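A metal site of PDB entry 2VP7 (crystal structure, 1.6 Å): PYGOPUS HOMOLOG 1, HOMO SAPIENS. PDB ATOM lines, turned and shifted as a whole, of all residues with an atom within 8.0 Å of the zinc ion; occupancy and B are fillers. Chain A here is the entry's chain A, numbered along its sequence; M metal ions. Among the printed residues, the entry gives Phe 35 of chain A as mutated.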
ATOM      1  N   PRO A  11     -15.588  35.227  -3.636  1.00  0.00           N
ATOM      2  CA  PRO A  11     -14.213  34.781  -3.537  1.00  0.00           C
ATOM      3  C   PRO A  11     -14.083  33.341  -3.064  1.00  0.00           C
ATOM      4  O   PRO A  11     -14.863  32.857  -2.226  1.00  0.00           O
ATOM      5  CB  PRO A  11     -13.634  35.745  -2.503  1.00  0.00           C
ATOM      6  CG  PRO A  11     -14.772  36.041  -1.608  1.00  0.00           C
ATOM      7  CD  PRO A  11     -16.002  36.005  -2.446  1.00  0.00           C
ATOM      8  N   CYS A  12     -13.062  32.652  -3.574  1.00  0.00           N
ATOM      9  CA  CYS A  12     -12.811  31.263  -3.219  1.00  0.00           C
ATOM     10  C   CYS A  12     -12.315  31.198  -1.793  1.00  0.00           C
ATOM     11  O   CYS A  12     -11.420  31.956  -1.393  1.00  0.00           O
ATOM     12  CB  CYS A  12     -11.759  30.669  -4.190  1.00  0.00           C
ATOM     13  SG  CYS A  12     -11.138  29.020  -3.805  1.00  0.00           S
ATOM     14  N   GLY A  13     -12.912  30.283  -1.022  1.00  0.00           N
ATOM     15  CA  GLY A  13     -12.526  30.047   0.383  1.00  0.00           C
ATOM     16  C   GLY A  13     -11.102  29.582   0.629  1.00  0.00           C
ATOM     17  O   GLY A  13     -10.610  29.629   1.772  1.00  0.00           O
ATOM     18  N   ILE A  14     -10.416  29.140  -0.444  1.00  0.00           N
ATOM     19  CA  ILE A  14      -9.015  28.738  -0.350  1.00  0.00           C
ATOM     20  C   ILE A  14      -8.019  29.786  -0.875  1.00  0.00           C
ATOM     21  O   ILE A  14      -7.104  30.192  -0.141  1.00  0.00           O
ATOM     22  CB  ILE A  14      -8.788  27.357  -1.040  1.00  0.00           C
ATOM     23  CG1 ILE A  14      -9.505  26.274  -0.233  1.00  0.00           C
ATOM     24  CG2 ILE A  14      -7.299  27.021  -1.149  1.00  0.00           C
ATOM     25  CD1 ILE A  14      -9.719  24.951  -1.016  1.00  0.00           C
ATOM     26  N   CYS A  15      -8.172  30.221  -2.123  1.00  0.00           N
ATOM     27  CA  CYS A  15      -7.183  31.112  -2.730  1.00  0.00           C
ATOM     28  C   CYS A  15      -7.514  32.612  -2.619  1.00  0.00           C
ATOM     29  O   CYS A  15      -6.644  33.457  -2.870  1.00  0.00           O
ATOM     30  CB  CYS A  15      -6.928  30.727  -4.199  1.00  0.00           C
ATOM     31  SG  CYS A  15      -8.259  31.139  -5.283  1.00  0.00           S
ATOM     32  N   THR A  16      -8.745  32.925  -2.209  1.00  0.00           N
ATOM     33  CA  THR A  16      -9.293  34.307  -2.156  1.00  0.00           C
ATOM     34  C   THR A  16      -9.652  34.977  -3.509  1.00  0.00           C
ATOM     35  O   THR A  16     -10.252  36.047  -3.530  1.00  0.00           O
ATOM     36  CB  THR A  16      -8.458  35.296  -1.283  1.00  0.00           C
ATOM     37  OG1 THR A  16      -7.316  35.741  -2.012  1.00  0.00           O
ATOM     38  CG2 THR A  16      -8.053  34.680   0.052  1.00  0.00           C
ATOM     39  N   ASN A  17      -9.318  34.321  -4.627  1.00  0.00           N
ATOM     40  CA  ASN A  17      -9.571  34.909  -5.943  1.00  0.00           C
ATOM     41  C   ASN A  17     -11.025  34.669  -6.330  1.00  0.00           C
ATOM     42  O   ASN A  17     -11.670  33.722  -5.827  1.00  0.00           O
ATOM     43  CB  ASN A  17      -8.619  34.310  -6.973  1.00  0.00           C
ATOM     44  CG  ASN A  17      -7.176  34.587  -6.642  1.00  0.00           C
ATOM     45  OD1 ASN A  17      -6.388  33.668  -6.484  1.00  0.00           O
ATOM     46  ND2 ASN A  17      -6.843  35.847  -6.478  1.00  0.00           N
ATOM     47  N   GLU A  18     -11.560  35.527  -7.197  1.00  0.00           N
ATOM     48  CA  GLU A  18     -12.969  35.414  -7.545  1.00  0.00           C
ATOM     49  C   GLU A  18     -13.241  34.075  -8.237  1.00  0.00           C
ATOM     50  O   GLU A  18     -12.413  33.596  -8.999  1.00  0.00           O
ATOM     51  CB  GLU A  18     -13.424  36.589  -8.406  1.00  0.00           C
ATOM     52  CG  GLU A  18     -13.462  37.922  -7.599  1.00  0.00           C
ATOM     53  CD  GLU A  18     -14.106  39.092  -8.353  1.00  0.00           C
ATOM     54  OE1 GLU A  18     -14.273  39.038  -9.587  1.00  0.00           O
ATOM     55  OE2 GLU A  18     -14.451  40.082  -7.683  1.00  0.00           O
ATOM     56  N   VAL A  19     -14.387  33.474  -7.935  1.00  0.00           N
ATOM     57  CA  VAL A  19     -14.827  32.296  -8.671  1.00  0.00           C
ATOM     58  C   VAL A  19     -15.690  32.789  -9.834  1.00  0.00           C
ATOM     59  O   VAL A  19     -16.869  33.155  -9.642  1.00  0.00           O
ATOM     60  CB  VAL A  19     -15.585  31.290  -7.778  1.00  0.00           C
ATOM     61  CG1 VAL A  19     -15.835  30.013  -8.546  1.00  0.00           C
ATOM     62  CG2 VAL A  19     -14.813  31.004  -6.496  1.00  0.00           C
ATOM     63  N   GLN A  23     -15.621  29.180 -14.573  1.00  0.00           N
ATOM     64  CA  GLN A  23     -14.832  28.292 -13.720  1.00  0.00           C
ATOM     65  C   GLN A  23     -15.774  27.396 -12.969  1.00  0.00           C
ATOM     66  O   GLN A  23     -16.876  27.827 -12.596  1.00  0.00           O
ATOM     67  CB  GLN A  23     -13.999  29.095 -12.709  1.00  0.00           C
ATOM     68  CG  GLN A  23     -12.777  29.818 -13.310  1.00  0.00           C
ATOM     69  CD  GLN A  23     -12.040  30.693 -12.326  1.00  0.00           C
ATOM     70  OE1 GLN A  23     -12.657  31.384 -11.520  1.00  0.00           O
ATOM     71  NE2 GLN A  23     -10.710  30.666 -12.377  1.00  0.00           N
ATOM     72  N   ASP A  24     -15.364  26.161 -12.720  1.00  0.00           N
ATOM     73  CA  ASP A  24     -16.204  25.266 -11.926  1.00  0.00           C
ATOM     74  C   ASP A  24     -16.167  25.770 -10.484  1.00  0.00           C
ATOM     75  O   ASP A  24     -15.080  25.908  -9.911  1.00  0.00           O
ATOM     76  CB  ASP A  24     -15.639  23.832 -11.936  1.00  0.00           C
ATOM     77  CG  ASP A  24     -15.853  23.103 -13.261  1.00  0.00           C
ATOM     78  OD1 ASP A  24     -16.730  23.497 -14.062  1.00  0.00           O
ATOM     79  OD2 ASP A  24     -15.154  22.076 -13.490  1.00  0.00           O
ATOM     80  N   PHE A  35     -18.063  29.576  -1.305  1.00  0.00           N
ATOM     81  CA  PHE A  35     -17.757  29.023  -2.626  1.00  0.00           C
ATOM     82  C   PHE A  35     -16.289  28.783  -2.781  1.00  0.00           C
ATOM     83  O   PHE A  35     -15.476  29.405  -2.098  1.00  0.00           O
ATOM     84  CB  PHE A  35     -18.202  29.963  -3.723  1.00  0.00           C
ATOM     85  CG  PHE A  35     -19.650  29.894  -4.001  1.00  0.00           C
ATOM     86  CD1 PHE A  35     -20.155  28.901  -4.830  1.00  0.00           C
ATOM     87  CD2 PHE A  35     -20.520  30.798  -3.396  1.00  0.00           C
ATOM     88  CE1 PHE A  35     -21.506  28.816  -5.099  1.00  0.00           C
ATOM     89  CE2 PHE A  35     -21.872  30.727  -3.637  1.00  0.00           C
ATOM     90  CZ  PHE A  35     -22.369  29.744  -4.497  1.00  0.00           C
ATOM     91  N   PHE A  36     -15.947  27.859  -3.678  1.00  0.00           N
ATOM     92  CA  PHE A  36     -14.550  27.469  -3.878  1.00  0.00           C
ATOM     93  C   PHE A  36     -14.405  27.093  -5.339  1.00  0.00           C
ATOM     94  O   PHE A  36     -15.306  26.534  -5.940  1.00  0.00           O
ATOM     95  CB  PHE A  36     -14.206  26.219  -3.076  1.00  0.00           C
ATOM     96  CG  PHE A  36     -14.318  26.359  -1.569  1.00  0.00           C
ATOM     97  CD1 PHE A  36     -13.176  26.457  -0.779  1.00  0.00           C
ATOM     98  CD2 PHE A  36     -15.561  26.313  -0.946  1.00  0.00           C
ATOM     99  CE1 PHE A  36     -13.281  26.543   0.621  1.00  0.00           C
ATOM    100  CE2 PHE A  36     -15.674  26.425   0.447  1.00  0.00           C
ATOM    101  CZ  PHE A  36     -14.541  26.530   1.212  1.00  0.00           C
ATOM    102  N   HIS A  37     -13.244  27.392  -5.911  1.00  0.00           N
ATOM    103  CA  HIS A  37     -12.879  26.773  -7.199  1.00  0.00           C
ATOM    104  C   HIS A  37     -12.756  25.262  -6.985  1.00  0.00           C
ATOM    105  O   HIS A  37     -12.061  24.796  -6.081  1.00  0.00           O
ATOM    106  CB  HIS A  37     -11.480  27.261  -7.695  1.00  0.00           C
ATOM    107  CG  HIS A  37     -11.373  28.735  -7.924  1.00  0.00           C
ATOM    108  ND1 HIS A  37     -10.659  29.562  -7.082  1.00  0.00           N
ATOM    109  CD2 HIS A  37     -11.805  29.509  -8.945  1.00  0.00           C
ATOM    110  CE1 HIS A  37     -10.726  30.803  -7.549  1.00  0.00           C
ATOM    111  NE2 HIS A  37     -11.402  30.787  -8.692  1.00  0.00           N
ATOM    112  N   ARG A  38     -13.404  24.494  -7.873  1.00  0.00           N
ATOM    113  CA  ARG A  38     -13.178  23.043  -7.907  1.00  0.00           C
ATOM    114  C   ARG A  38     -11.695  22.735  -7.862  1.00  0.00           C
ATOM    115  O   ARG A  38     -11.258  21.949  -7.053  1.00  0.00           O
ATOM    116  CB  ARG A  38     -13.805  22.407  -9.150  1.00  0.00           C
ATOM    117  CG  ARG A  38     -13.601  20.909  -9.166  1.00  0.00           C
ATOM    118  CD  ARG A  38     -13.856  20.250 -10.498  1.00  0.00           C
ATOM    119  NE  ARG A  38     -13.124  20.869 -11.630  1.00  0.00           N
ATOM    120  CZ  ARG A  38     -11.829  20.664 -11.881  1.00  0.00           C
ATOM    121  NH1 ARG A  38     -11.064  19.892 -11.114  1.00  0.00           N
ATOM    122  NH2 ARG A  38     -11.287  21.234 -12.964  1.00  0.00           N
ATOM    123  N   ILE A  39     -10.907  23.408  -8.702  1.00  0.00           N
ATOM    124  CA  ILE A  39      -9.466  23.173  -8.779  1.00  0.00           C
ATOM    125  C   ILE A  39      -8.786  23.259  -7.406  1.00  0.00           C
ATOM    126  O   ILE A  39      -7.946  22.416  -7.024  1.00  0.00           O
ATOM    127  CB  ILE A  39      -8.853  24.164  -9.788  1.00  0.00           C
ATOM    128  CG1 ILE A  39      -9.267  23.763 -11.211  1.00  0.00           C
ATOM    129  CG2 ILE A  39      -7.338  24.226  -9.648  1.00  0.00           C
ATOM    130  CD1 ILE A  39      -9.226  24.908 -12.203  1.00  0.00           C
ATOM    131  N   CYS A  40      -9.145  24.309  -6.655  1.00  0.00           N
ATOM    132  CA  CYS A  40      -8.545  24.558  -5.361  1.00  0.00           C
ATOM    133  C   CYS A  40      -8.844  23.460  -4.312  1.00  0.00           C
ATOM    134  O   CYS A  40      -8.054  23.249  -3.399  1.00  0.00           O
ATOM    135  CB  CYS A  40      -8.952  25.943  -4.856  1.00  0.00           C
ATOM    136  SG  CYS A  40      -8.297  27.278  -5.894  1.00  0.00           S
ATOM    137  N   THR A  41      -9.995  22.795  -4.437  1.00  0.00           N
ATOM    138  CA  THR A  41     -10.377  21.782  -3.470  1.00  0.00           C
ATOM    139  C   THR A  41      -9.645  20.445  -3.710  1.00  0.00           C
ATOM    140  O   THR A  41      -9.536  19.620  -2.810  1.00  0.00           O
ATOM    141  CB  THR A  41     -11.899  21.493  -3.542  1.00  0.00           C
ATOM    142  OG1 THR A  41     -12.194  20.831  -4.777  1.00  0.00           O
ATOM    143  CG2 THR A  41     -12.693  22.756  -3.384  1.00  0.00           C
HETATM  144 ZN    ZN M   1      -9.554  29.111  -5.491  1.00  0.00          ZN
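ND1 of His 37 is bound to the zinc ion (2.0 Å).
The side-chain sulfur (SG) of Cys 40 binds the zinc ion (2.3 Å).
SG of Cys 12 binds the zinc ion (2.3 Å).
The zinc ion is bound by SG of Cys 15, 2.4 Å away.
The zinc ion has four donor atoms within binding distance.
A ring nitrogen (NE2) of His 37 lies within hydrogen-bond range of the backbone carbonyl oxygen of Glu 18, at 3.0 Å.
The side-chain sulfur (SG) of Cys 12 lies close to the backbone NH (N) of Ile 14 (3.4 Å).
N of Cys 12 is in hydrogen-bond range of O of Asn 17, at 2.9 Å.
The side-chain amide oxygen of Gln 23 sits at hydrogen-bond distance from a ring nitrogen (NE2) of His 37 (3.2 Å).
The side-chain sulfur (SG) of Cys 15 lies close to the side-chain amide oxygen (OD1) of Asn 17 (3.4 Å).
Of the 18 residues printed, 4 come within 4 Å of the zinc ion.
The nearest printed residue that does not touch the zinc ion is Ile 14 (4.8 Å).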
